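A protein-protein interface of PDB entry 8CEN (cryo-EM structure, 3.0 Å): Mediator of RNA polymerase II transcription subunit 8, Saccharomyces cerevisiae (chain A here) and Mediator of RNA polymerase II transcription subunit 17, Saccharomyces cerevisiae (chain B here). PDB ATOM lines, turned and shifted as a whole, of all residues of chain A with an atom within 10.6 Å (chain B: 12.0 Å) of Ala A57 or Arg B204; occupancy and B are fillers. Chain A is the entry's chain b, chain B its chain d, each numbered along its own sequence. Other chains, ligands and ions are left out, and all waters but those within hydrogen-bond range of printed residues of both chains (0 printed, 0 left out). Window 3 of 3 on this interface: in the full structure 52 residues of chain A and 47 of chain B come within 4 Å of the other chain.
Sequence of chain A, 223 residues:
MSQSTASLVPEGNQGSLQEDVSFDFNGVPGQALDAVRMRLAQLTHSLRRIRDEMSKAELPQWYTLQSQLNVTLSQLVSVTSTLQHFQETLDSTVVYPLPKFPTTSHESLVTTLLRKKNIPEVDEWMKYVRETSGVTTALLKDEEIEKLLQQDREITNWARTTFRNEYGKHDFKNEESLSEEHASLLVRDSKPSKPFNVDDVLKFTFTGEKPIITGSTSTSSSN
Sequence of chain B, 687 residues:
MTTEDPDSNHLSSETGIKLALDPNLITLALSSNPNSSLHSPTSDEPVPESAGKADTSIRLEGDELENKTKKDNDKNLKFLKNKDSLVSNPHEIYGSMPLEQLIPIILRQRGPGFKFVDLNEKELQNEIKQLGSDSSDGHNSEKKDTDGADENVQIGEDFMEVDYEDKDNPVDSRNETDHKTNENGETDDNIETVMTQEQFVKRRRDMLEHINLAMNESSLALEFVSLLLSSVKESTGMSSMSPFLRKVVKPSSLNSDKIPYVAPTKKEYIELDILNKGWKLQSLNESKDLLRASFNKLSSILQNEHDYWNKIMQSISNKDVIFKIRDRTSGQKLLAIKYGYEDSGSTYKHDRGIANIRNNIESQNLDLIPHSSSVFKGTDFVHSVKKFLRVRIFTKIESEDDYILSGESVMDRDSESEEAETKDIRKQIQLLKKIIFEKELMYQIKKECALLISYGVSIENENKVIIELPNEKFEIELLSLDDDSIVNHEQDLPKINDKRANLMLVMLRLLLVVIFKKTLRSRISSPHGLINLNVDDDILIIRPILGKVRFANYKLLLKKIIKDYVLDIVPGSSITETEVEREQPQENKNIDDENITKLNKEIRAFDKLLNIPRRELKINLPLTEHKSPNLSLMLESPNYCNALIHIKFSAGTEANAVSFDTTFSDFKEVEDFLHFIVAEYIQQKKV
NH2 of Arg B204 lies within hydrogen-bond range of O of Lys A56.
The side-chain hydroxyl of Ser A55 sits at hydrogen-bond distance from the backbone carbonyl oxygen of Arg A51 (3.2 Å).
The side-chain carboxylate (OE2) of Glu A53 is in salt-bridge range of the side-chain amino group (NZ) of Lys A56.
O of Leu B208 lies within hydrogen-bond range of ND2 of Asn B212 (3.0 Å).
Among the printed residues, pairs that only touch across the chains: Arg A51 with Asn B212 (3.2 Å), Met A54 with Met B207 (3.6 Å), Ala A57 with Arg B204 (3.6 Å), Ser A55 with Leu B208 (3.6 Å), Ile A50 with Ile B211 (3.7 Å), Leu A59 with Arg B204 (3.7 Å), Ser A55 with Arg B204 (3.7 Å) and Met A54 with Arg B204 (3.9 Å).
Of the printed residues of chain B, Ile A50 touches Ile B211 (3.7 Å).
Printed residues of chain B within 4 Å of Arg A51: Asn B212.
Glu A53 touches none of the printed residues of chain B.
Met A54 touches two residues of chain B.
Of chain B, only Arg B204 (3.7 Å) and Leu B208 (3.6 Å) come within 4 Å of Ser A55.
Of chain B, only Arg B204 comes within 4 Å of Lys A56.
Of chain B, only Arg B204 comes within 4 Å of Ala A57.
No residue of chain B comes within 4 Å of Glu A58.
No residue of chain A comes within 4 Å of Val B201.
Arg B204 touches just these residues of chain A: Met A54 (3.9 Å), Ser A55 (3.7 Å), Lys A56 (3.0 Å), Ala A57 (3.6 Å) and Leu A59 (3.7 Å).
Met B207 touches just one residue of chain A: Met A54 (3.6 Å).
Of the printed residues of chain A, Ile B211 touches Ile A50.
Printed residues of chain A within 4 Å of Asn B212: Arg A51.
The nearest printed residue of chain A that does not touch Asn B212 is Ser A55 (6.3 Å).
Hydrophobic or aromatic side chains of chain B that line the printed part of chain A: Met B207, Leu B208 and Ile B211.
Of the 13 printed residues of chain A, 7 touch a printed residue of chain B.
Among the printed residues, 9 pairs touch across the chains.
Among the printed residues, no Asp or Glu carboxylate lies within 4 Å of a Lys or Arg side-chain nitrogen of the other chain.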
ATOM      1  N   ILE A  50      37.043 -25.498 -18.920  1.00  0.00           N
ATOM      2  CA  ILE A  50      35.690 -25.656 -19.446  1.00  0.00           C
ATOM      3  C   ILE A  50      35.670 -26.691 -20.564  1.00  0.00           C
ATOM      4  O   ILE A  50      34.772 -27.542 -20.616  1.00  0.00           O
ATOM      5  CB  ILE A  50      35.126 -24.299 -19.905  1.00  0.00           C
ATOM      6  CG1 ILE A  50      34.994 -23.354 -18.714  1.00  0.00           C
ATOM      7  CG2 ILE A  50      33.761 -24.467 -20.539  1.00  0.00           C
ATOM      8  CD1 ILE A  50      34.559 -21.967 -19.099  1.00  0.00           C
ATOM      9  N   ARG A  51      36.687 -26.673 -21.435  1.00  0.00           N
ATOM     10  CA  ARG A  51      36.797 -27.660 -22.509  1.00  0.00           C
ATOM     11  C   ARG A  51      36.864 -29.078 -21.948  1.00  0.00           C
ATOM     12  O   ARG A  51      36.011 -29.920 -22.249  1.00  0.00           O
ATOM     13  CB  ARG A  51      38.031 -27.365 -23.380  1.00  0.00           C
ATOM     14  CG  ARG A  51      38.205 -28.242 -24.657  1.00  0.00           C
ATOM     15  CD  ARG A  51      38.947 -29.581 -24.442  1.00  0.00           C
ATOM     16  NE  ARG A  51      40.274 -29.429 -23.861  1.00  0.00           N
ATOM     17  CZ  ARG A  51      41.364 -29.135 -24.552  1.00  0.00           C
ATOM     18  NH1 ARG A  51      41.350 -29.082 -25.872  1.00  0.00           N
ATOM     19  NH2 ARG A  51      42.507 -28.930 -23.904  1.00  0.00           N
ATOM     20  N   ASP A  52      37.890 -29.370 -21.144  1.00  0.00           N
ATOM     21  CA  ASP A  52      38.099 -30.761 -20.759  1.00  0.00           C
ATOM     22  C   ASP A  52      37.183 -31.217 -19.630  1.00  0.00           C
ATOM     23  O   ASP A  52      37.201 -32.403 -19.284  1.00  0.00           O
ATOM     24  CB  ASP A  52      39.574 -31.025 -20.403  1.00  0.00           C
ATOM     25  CG  ASP A  52      40.118 -30.108 -19.313  1.00  0.00           C
ATOM     26  OD1 ASP A  52      39.342 -29.473 -18.572  1.00  0.00           O
ATOM     27  OD2 ASP A  52      41.359 -30.025 -19.200  1.00  0.00           O
ATOM     28  N   GLU A  53      36.388 -30.317 -19.050  1.00  0.00           N
ATOM     29  CA  GLU A  53      35.361 -30.707 -18.096  1.00  0.00           C
ATOM     30  C   GLU A  53      33.999 -30.866 -18.756  1.00  0.00           C
ATOM     31  O   GLU A  53      33.191 -31.689 -18.315  1.00  0.00           O
ATOM     32  CB  GLU A  53      35.285 -29.658 -16.974  1.00  0.00           C
ATOM     33  CG  GLU A  53      34.193 -29.830 -15.917  1.00  0.00           C
ATOM     34  CD  GLU A  53      34.303 -31.140 -15.146  1.00  0.00           C
ATOM     35  OE1 GLU A  53      34.923 -31.132 -14.062  1.00  0.00           O
ATOM     36  OE2 GLU A  53      33.758 -32.168 -15.598  1.00  0.00           O
ATOM     37  N   MET A  54      33.753 -30.143 -19.848  1.00  0.00           N
ATOM     38  CA  MET A  54      32.445 -30.079 -20.466  1.00  0.00           C
ATOM     39  C   MET A  54      32.354 -30.915 -21.739  1.00  0.00           C
ATOM     40  O   MET A  54      31.243 -31.196 -22.203  1.00  0.00           O
ATOM     41  CB  MET A  54      32.131 -28.596 -20.739  1.00  0.00           C
ATOM     42  CG  MET A  54      30.786 -28.212 -21.307  1.00  0.00           C
ATOM     43  SD  MET A  54      30.770 -26.413 -21.384  1.00  0.00           S
ATOM     44  CE  MET A  54      29.200 -26.089 -22.155  1.00  0.00           C
ATOM     45  N   SER A  55      33.490 -31.367 -22.283  1.00  0.00           N
ATOM     46  CA  SER A  55      33.476 -32.251 -23.443  1.00  0.00           C
ATOM     47  C   SER A  55      33.037 -33.669 -23.101  1.00  0.00           C
ATOM     48  O   SER A  55      32.739 -34.445 -24.016  1.00  0.00           O
ATOM     49  CB  SER A  55      34.863 -32.302 -24.083  1.00  0.00           C
ATOM     50  OG  SER A  55      35.788 -32.957 -23.236  1.00  0.00           O
ATOM     51  N   LYS A  56      33.008 -34.029 -21.821  1.00  0.00           N
ATOM     52  CA  LYS A  56      32.660 -35.385 -21.425  1.00  0.00           C
ATOM     53  C   LYS A  56      31.175 -35.655 -21.659  1.00  0.00           C
ATOM     54  O   LYS A  56      30.365 -34.739 -21.829  1.00  0.00           O
ATOM     55  CB  LYS A  56      33.015 -35.620 -19.957  1.00  0.00           C
ATOM     56  CG  LYS A  56      34.479 -35.365 -19.628  1.00  0.00           C
ATOM     57  CD  LYS A  56      34.677 -34.974 -18.170  1.00  0.00           C
ATOM     58  CE  LYS A  56      34.019 -35.966 -17.227  1.00  0.00           C
ATOM     59  NZ  LYS A  56      34.344 -35.676 -15.804  1.00  0.00           N
ATOM     60  N   ALA A  57      30.827 -36.945 -21.678  1.00  0.00           N
ATOM     61  CA  ALA A  57      29.451 -37.351 -21.938  1.00  0.00           C
ATOM     62  C   ALA A  57      28.505 -36.972 -20.807  1.00  0.00           C
ATOM     63  O   ALA A  57      27.305 -36.810 -21.048  1.00  0.00           O
ATOM     64  CB  ALA A  57      29.387 -38.859 -22.185  1.00  0.00           C
ATOM     65  N   GLU A  58      29.013 -36.825 -19.587  1.00  0.00           N
ATOM     66  CA  GLU A  58      28.211 -36.425 -18.441  1.00  0.00           C
ATOM     67  C   GLU A  58      28.629 -35.029 -18.006  1.00  0.00           C
ATOM     68  O   GLU A  58      29.814 -34.779 -17.762  1.00  0.00           O
ATOM     69  CB  GLU A  58      28.371 -37.419 -17.288  1.00  0.00           C
ATOM     70  CG  GLU A  58      27.306 -37.298 -16.211  1.00  0.00           C
ATOM     71  CD  GLU A  58      27.789 -36.527 -14.998  1.00  0.00           C
ATOM     72  OE1 GLU A  58      29.014 -36.322 -14.872  1.00  0.00           O
ATOM     73  OE2 GLU A  58      26.944 -36.128 -14.170  1.00  0.00           O
ATOM     74  N   LEU A  59      27.657 -34.125 -17.922  1.00  0.00           N
ATOM     75  CA  LEU A  59      27.943 -32.743 -17.576  1.00  0.00           C
ATOM     76  C   LEU A  59      28.331 -32.628 -16.102  1.00  0.00           C
ATOM     77  O   LEU A  59      27.864 -33.406 -15.266  1.00  0.00           O
ATOM     78  CB  LEU A  59      26.732 -31.851 -17.853  1.00  0.00           C
ATOM     79  CG  LEU A  59      26.472 -31.284 -19.254  1.00  0.00           C
ATOM     80  CD1 LEU A  59      27.607 -30.355 -19.677  1.00  0.00           C
ATOM     81  CD2 LEU A  59      26.221 -32.361 -20.302  1.00  0.00           C
ATOM     82  N   PRO A  60      29.183 -31.665 -15.757  1.00  0.00           N
ATOM     83  CA  PRO A  60      29.451 -31.387 -14.343  1.00  0.00           C
ATOM     84  C   PRO A  60      28.237 -30.764 -13.673  1.00  0.00           C
ATOM     85  O   PRO A  60      27.250 -30.403 -14.317  1.00  0.00           O
ATOM     86  CB  PRO A  60      30.630 -30.412 -14.391  1.00  0.00           C
ATOM     87  CG  PRO A  60      30.500 -29.751 -15.721  1.00  0.00           C
ATOM     88  CD  PRO A  60      30.018 -30.834 -16.642  1.00  0.00           C
ATOM     89  N   GLN A  61      28.316 -30.660 -12.347  1.00  0.00           N
ATOM     90  CA  GLN A  61      27.239 -30.045 -11.583  1.00  0.00           C
ATOM     91  C   GLN A  61      27.102 -28.576 -11.967  1.00  0.00           C
ATOM     92  O   GLN A  61      28.100 -27.872 -12.156  1.00  0.00           O
ATOM     93  CB  GLN A  61      27.501 -30.191 -10.082  1.00  0.00           C
ATOM     94  CG  GLN A  61      26.389 -29.649  -9.200  1.00  0.00           C
ATOM     95  CD  GLN A  61      25.075 -30.378  -9.413  1.00  0.00           C
ATOM     96  OE1 GLN A  61      24.158 -29.857 -10.048  1.00  0.00           O
ATOM     97  NE2 GLN A  61      24.980 -31.593  -8.885  1.00  0.00           N
ATOM     98  N   LEU A  65      29.760 -25.544 -12.729  1.00  0.00           N
ATOM     99  CA  LEU A  65      29.922 -25.068 -14.099  1.00  0.00           C
ATOM    100  C   LEU A  65      29.639 -23.575 -14.208  1.00  0.00           C
ATOM    101  O   LEU A  65      30.360 -22.852 -14.904  1.00  0.00           O
ATOM    102  CB  LEU A  65      29.013 -25.856 -15.042  1.00  0.00           C
ATOM    103  CG  LEU A  65      29.212 -25.627 -16.542  1.00  0.00           C
ATOM    104  CD1 LEU A  65      30.687 -25.655 -16.914  1.00  0.00           C
ATOM    105  CD2 LEU A  65      28.434 -26.655 -17.349  1.00  0.00           C
ATOM    106  N   MET B 195      11.820 -31.331 -25.339  1.00  0.00           N
ATOM    107  CA  MET B 195      13.211 -31.391 -25.765  1.00  0.00           C
ATOM    108  C   MET B 195      13.634 -32.846 -25.909  1.00  0.00           C
ATOM    109  O   MET B 195      13.334 -33.677 -25.046  1.00  0.00           O
ATOM    110  CB  MET B 195      14.101 -30.646 -24.760  1.00  0.00           C
ATOM    111  CG  MET B 195      15.589 -30.552 -25.090  1.00  0.00           C
ATOM    112  SD  MET B 195      16.603 -31.979 -24.668  1.00  0.00           S
ATOM    113  CE  MET B 195      16.641 -31.828 -22.889  1.00  0.00           C
ATOM    114  N   THR B 196      14.340 -33.148 -26.995  1.00  0.00           N
ATOM    115  CA  THR B 196      14.677 -34.518 -27.348  1.00  0.00           C
ATOM    116  C   THR B 196      16.188 -34.722 -27.366  1.00  0.00           C
ATOM    117  O   THR B 196      16.975 -33.771 -27.324  1.00  0.00           O
ATOM    118  CB  THR B 196      14.074 -34.900 -28.706  1.00  0.00           C
ATOM    119  OG1 THR B 196      14.348 -36.280 -28.982  1.00  0.00           O
ATOM    120  CG2 THR B 196      14.659 -34.038 -29.810  1.00  0.00           C
ATOM    121  N   GLN B 197      16.571 -36.001 -27.434  1.00  0.00           N
ATOM    122  CA  GLN B 197      17.971 -36.404 -27.307  1.00  0.00           C
ATOM    123  C   GLN B 197      18.824 -35.890 -28.462  1.00  0.00           C
ATOM    124  O   GLN B 197      19.964 -35.464 -28.250  1.00  0.00           O
ATOM    125  CB  GLN B 197      18.055 -37.928 -27.216  1.00  0.00           C
ATOM    126  CG  GLN B 197      19.456 -38.483 -27.011  1.00  0.00           C
ATOM    127  CD  GLN B 197      20.090 -38.029 -25.712  1.00  0.00           C
ATOM    128  OE1 GLN B 197      20.967 -37.168 -25.705  1.00  0.00           O
ATOM    129  NE2 GLN B 197      19.652 -38.615 -24.602  1.00  0.00           N
ATOM    130  N   GLU B 198      18.301 -35.930 -29.690  1.00  0.00           N
ATOM    131  CA  GLU B 198      19.089 -35.503 -30.845  1.00  0.00           C
ATOM    132  C   GLU B 198      19.303 -33.990 -30.857  1.00  0.00           C
ATOM    133  O   GLU B 198      20.401 -33.514 -31.180  1.00  0.00           O
ATOM    134  CB  GLU B 198      18.424 -36.015 -32.129  1.00  0.00           C
ATOM    135  CG  GLU B 198      16.955 -35.637 -32.314  1.00  0.00           C
ATOM    136  CD  GLU B 198      16.761 -34.357 -33.091  1.00  0.00           C
ATOM    137  OE1 GLU B 198      17.697 -33.961 -33.813  1.00  0.00           O
ATOM    138  OE2 GLU B 198      15.678 -33.745 -32.980  1.00  0.00           O
ATOM    139  N   GLN B 199      18.285 -33.220 -30.468  1.00  0.00           N
ATOM    140  CA  GLN B 199      18.458 -31.777 -30.328  1.00  0.00           C
ATOM    141  C   GLN B 199      19.416 -31.454 -29.185  1.00  0.00           C
ATOM    142  O   GLN B 199      20.253 -30.545 -29.299  1.00  0.00           O
ATOM    143  CB  GLN B 199      17.095 -31.119 -30.122  1.00  0.00           C
ATOM    144  CG  GLN B 199      17.086 -29.610 -30.245  1.00  0.00           C
ATOM    145  CD  GLN B 199      15.712 -29.027 -29.976  1.00  0.00           C
ATOM    146  OE1 GLN B 199      14.785 -29.744 -29.599  1.00  0.00           O
ATOM    147  NE2 GLN B 199      15.570 -27.722 -30.181  1.00  0.00           N
ATOM    148  N   PHE B 200      19.326 -32.220 -28.092  1.00  0.00           N
ATOM    149  CA  PHE B 200      20.247 -32.068 -26.971  1.00  0.00           C
ATOM    150  C   PHE B 200      21.687 -32.328 -27.393  1.00  0.00           C
ATOM    151  O   PHE B 200      22.594 -31.571 -27.027  1.00  0.00           O
ATOM    152  CB  PHE B 200      19.833 -33.015 -25.842  1.00  0.00           C
ATOM    153  CG  PHE B 200      20.833 -33.125 -24.726  1.00  0.00           C
ATOM    154  CD1 PHE B 200      20.908 -32.150 -23.747  1.00  0.00           C
ATOM    155  CD2 PHE B 200      21.672 -34.225 -24.636  1.00  0.00           C
ATOM    156  CE1 PHE B 200      21.821 -32.256 -22.713  1.00  0.00           C
ATOM    157  CE2 PHE B 200      22.587 -34.337 -23.606  1.00  0.00           C
ATOM    158  CZ  PHE B 200      22.661 -33.351 -22.644  1.00  0.00           C
ATOM    159  N   VAL B 201      21.916 -33.376 -28.185  1.00  0.00           N
ATOM    160  CA  VAL B 201      23.289 -33.719 -28.529  1.00  0.00           C
ATOM    161  C   VAL B 201      23.839 -32.783 -29.606  1.00  0.00           C
ATOM    162  O   VAL B 201      25.045 -32.508 -29.621  1.00  0.00           O
ATOM    163  CB  VAL B 201      23.412 -35.207 -28.923  1.00  0.00           C
ATOM    164  CG1 VAL B 201      22.800 -35.498 -30.285  1.00  0.00           C
ATOM    165  CG2 VAL B 201      24.869 -35.664 -28.866  1.00  0.00           C
ATOM    166  N   LYS B 202      22.994 -32.227 -30.489  1.00  0.00           N
ATOM    167  CA  LYS B 202      23.539 -31.233 -31.413  1.00  0.00           C
ATOM    168  C   LYS B 202      23.842 -29.917 -30.703  1.00  0.00           C
ATOM    169  O   LYS B 202      24.827 -29.246 -31.043  1.00  0.00           O
ATOM    170  CB  LYS B 202      22.634 -30.995 -32.626  1.00  0.00           C
ATOM    171  CG  LYS B 202      21.275 -30.384 -32.382  1.00  0.00           C
ATOM    172  CD  LYS B 202      20.569 -30.180 -33.715  1.00  0.00           C
ATOM    173  CE  LYS B 202      20.118 -31.481 -34.343  1.00  0.00           C
ATOM    174  NZ  LYS B 202      19.071 -32.148 -33.554  1.00  0.00           N
ATOM    175  N   ARG B 203      23.034 -29.534 -29.703  1.00  0.00           N
ATOM    176  CA  ARG B 203      23.404 -28.373 -28.895  1.00  0.00           C
ATOM    177  C   ARG B 203      24.687 -28.631 -28.114  1.00  0.00           C
ATOM    178  O   ARG B 203      25.537 -27.740 -27.996  1.00  0.00           O
ATOM    179  CB  ARG B 203      22.274 -27.975 -27.946  1.00  0.00           C
ATOM    180  CG  ARG B 203      21.309 -26.962 -28.536  1.00  0.00           C
ATOM    181  CD  ARG B 203      20.306 -26.507 -27.498  1.00  0.00           C
ATOM    182  NE  ARG B 203      19.352 -27.552 -27.151  1.00  0.00           N
ATOM    183  CZ  ARG B 203      18.070 -27.536 -27.483  1.00  0.00           C
ATOM    184  NH1 ARG B 203      17.547 -26.536 -28.173  1.00  0.00           N
ATOM    185  NH2 ARG B 203      17.290 -28.541 -27.101  1.00  0.00           N
ATOM    186  N   ARG B 204      24.853 -29.855 -27.600  1.00  0.00           N
ATOM    187  CA  ARG B 204      26.080 -30.225 -26.901  1.00  0.00           C
ATOM    188  C   ARG B 204      27.293 -30.113 -27.815  1.00  0.00           C
ATOM    189  O   ARG B 204      28.319 -29.534 -27.434  1.00  0.00           O
ATOM    190  CB  ARG B 204      25.953 -31.654 -26.366  1.00  0.00           C
ATOM    191  CG  ARG B 204      25.231 -31.770 -25.034  1.00  0.00           C
ATOM    192  CD  ARG B 204      26.170 -31.504 -23.874  1.00  0.00           C
ATOM    193  NE  ARG B 204      27.513 -32.022 -24.106  1.00  0.00           N
ATOM    194  CZ  ARG B 204      27.864 -33.291 -23.946  1.00  0.00           C
ATOM    195  NH1 ARG B 204      27.023 -34.184 -23.450  1.00  0.00           N
ATOM    196  NH2 ARG B 204      29.097 -33.667 -24.268  1.00  0.00           N
ATOM    197  N   ARG B 205      27.171 -30.622 -29.044  1.00  0.00           N
ATOM    198  CA  ARG B 205      28.283 -30.590 -29.989  1.00  0.00           C
ATOM    199  C   ARG B 205      28.610 -29.167 -30.427  1.00  0.00           C
ATOM    200  O   ARG B 205      29.790 -28.805 -30.535  1.00  0.00           O
ATOM    201  CB  ARG B 205      27.962 -31.470 -31.196  1.00  0.00           C
ATOM    202  CG  ARG B 205      29.101 -31.613 -32.186  1.00  0.00           C
ATOM    203  CD  ARG B 205      28.723 -32.562 -33.310  1.00  0.00           C
ATOM    204  NE  ARG B 205      27.621 -32.048 -34.113  1.00  0.00           N
ATOM    205  CZ  ARG B 205      26.416 -32.598 -34.169  1.00  0.00           C
ATOM    206  NH1 ARG B 205      26.124 -33.689 -33.481  1.00  0.00           N
ATOM    207  NH2 ARG B 205      25.480 -32.038 -34.929  1.00  0.00           N
ATOM    208  N   ASP B 206      27.591 -28.335 -30.672  1.00  0.00           N
ATOM    209  CA  ASP B 206      27.896 -26.987 -31.136  1.00  0.00           C
ATOM    210  C   ASP B 206      28.459 -26.115 -30.017  1.00  0.00           C
ATOM    211  O   ASP B 206      29.340 -25.286 -30.273  1.00  0.00           O
ATOM    212  CB  ASP B 206      26.676 -26.354 -31.837  1.00  0.00           C
ATOM    213  CG  ASP B 206      25.479 -26.077 -30.912  1.00  0.00           C
ATOM    214  OD1 ASP B 206      25.620 -25.566 -29.782  1.00  0.00           O
ATOM    215  OD2 ASP B 206      24.349 -26.361 -31.359  1.00  0.00           O
ATOM    216  N   MET B 207      28.017 -26.308 -28.768  1.00  0.00           N
ATOM    217  CA  MET B 207      28.648 -25.533 -27.703  1.00  0.00           C
ATOM    218  C   MET B 207      30.044 -26.057 -27.390  1.00  0.00           C
ATOM    219  O   MET B 207      30.923 -25.270 -27.012  1.00  0.00           O
ATOM    220  CB  MET B 207      27.771 -25.492 -26.450  1.00  0.00           C
ATOM    221  CG  MET B 207      27.514 -26.768 -25.693  1.00  0.00           C
ATOM    222  SD  MET B 207      26.405 -26.337 -24.334  1.00  0.00           S
ATOM    223  CE  MET B 207      26.171 -27.912 -23.532  1.00  0.00           C
ATOM    224  N   LEU B 208      30.286 -27.358 -27.590  1.00  0.00           N
ATOM    225  CA  LEU B 208      31.645 -27.882 -27.486  1.00  0.00           C
ATOM    226  C   LEU B 208      32.564 -27.270 -28.539  1.00  0.00           C
ATOM    227  O   LEU B 208      33.698 -26.885 -28.233  1.00  0.00           O
ATOM    228  CB  LEU B 208      31.627 -29.407 -27.601  1.00  0.00           C
ATOM    229  CG  LEU B 208      32.960 -30.112 -27.863  1.00  0.00           C
ATOM    230  CD1 LEU B 208      33.901 -29.945 -26.686  1.00  0.00           C
ATOM    231  CD2 LEU B 208      32.730 -31.590 -28.161  1.00  0.00           C
ATOM    232  N   GLU B 209      32.088 -27.143 -29.781  1.00  0.00           N
ATOM    233  CA  GLU B 209      32.959 -26.568 -30.803  1.00  0.00           C
ATOM    234  C   GLU B 209      33.129 -25.063 -30.614  1.00  0.00           C
ATOM    235  O   GLU B 209      34.199 -24.522 -30.919  1.00  0.00           O
ATOM    236  CB  GLU B 209      32.452 -26.904 -32.211  1.00  0.00           C
ATOM    237  CG  GLU B 209      31.280 -26.092 -32.729  1.00  0.00           C
ATOM    238  CD  GLU B 209      30.938 -26.427 -34.168  1.00  0.00           C
ATOM    239  OE1 GLU B 209      31.577 -27.338 -34.736  1.00  0.00           O
ATOM    240  OE2 GLU B 209      30.037 -25.774 -34.737  1.00  0.00           O
ATOM    241  N   HIS B 210      32.117 -24.374 -30.070  1.00  0.00           N
ATOM    242  CA  HIS B 210      32.280 -22.953 -29.774  1.00  0.00           C
ATOM    243  C   HIS B 210      33.272 -22.727 -28.638  1.00  0.00           C
ATOM    244  O   HIS B 210      34.075 -21.785 -28.690  1.00  0.00           O
ATOM    245  CB  HIS B 210      30.930 -22.316 -29.449  1.00  0.00           C
ATOM    246  CG  HIS B 210      30.044 -22.131 -30.642  1.00  0.00           C
ATOM    247  ND1 HIS B 210      29.142 -23.086 -31.057  1.00  0.00           N
ATOM    248  CD2 HIS B 210      29.927 -21.100 -31.511  1.00  0.00           C
ATOM    249  CE1 HIS B 210      28.504 -22.650 -32.129  1.00  0.00           C
ATOM    250  NE2 HIS B 210      28.962 -21.448 -32.426  1.00  0.00           N
ATOM    251  N   ILE B 211      33.248 -23.579 -27.606  1.00  0.00           N
ATOM    252  CA  ILE B 211      34.231 -23.421 -26.538  1.00  0.00           C
ATOM    253  C   ILE B 211      35.623 -23.825 -27.024  1.00  0.00           C
ATOM    254  O   ILE B 211      36.629 -23.255 -26.576  1.00  0.00           O
ATOM    255  CB  ILE B 211      33.794 -24.179 -25.263  1.00  0.00           C
ATOM    256  CG1 ILE B 211      34.410 -23.526 -24.028  1.00  0.00           C
ATOM    257  CG2 ILE B 211      34.165 -25.653 -25.286  1.00  0.00           C
ATOM    258  CD1 ILE B 211      34.006 -22.090 -23.846  1.00  0.00           C
ATOM    259  N   ASN B 212      35.706 -24.766 -27.976  1.00  0.00           N
ATOM    260  CA  ASN B 212      36.989 -25.085 -28.599  1.00  0.00           C
ATOM    261  C   ASN B 212      37.546 -23.889 -29.357  1.00  0.00           C
ATOM    262  O   ASN B 212      38.738 -23.580 -29.255  1.00  0.00           O
ATOM    263  CB  ASN B 212      36.839 -26.277 -29.544  1.00  0.00           C
ATOM    264  CG  ASN B 212      36.691 -27.592 -28.812  1.00  0.00           C
ATOM    265  OD1 ASN B 212      37.214 -27.765 -27.714  1.00  0.00           O
ATOM    266  ND2 ASN B 212      35.975 -28.530 -29.420  1.00  0.00           N
ATOM    267  N   LEU B 213      36.690 -23.199 -30.116  1.00  0.00           N
ATOM    268  CA  LEU B 213      37.136 -22.027 -30.863  1.00  0.00           C
ATOM    269  C   LEU B 213      37.542 -20.889 -29.932  1.00  0.00           C
ATOM    270  O   LEU B 213      38.530 -20.190 -30.198  1.00  0.00           O
ATOM    271  CB  LEU B 213      36.039 -21.577 -31.827  1.00  0.00           C
ATOM    272  CG  LEU B 213      35.769 -22.515 -33.004  1.00  0.00           C
ATOM    273  CD1 LEU B 213      34.518 -22.092 -33.755  1.00  0.00           C
ATOM    274  CD2 LEU B 213      36.969 -22.566 -33.937  1.00  0.00           C
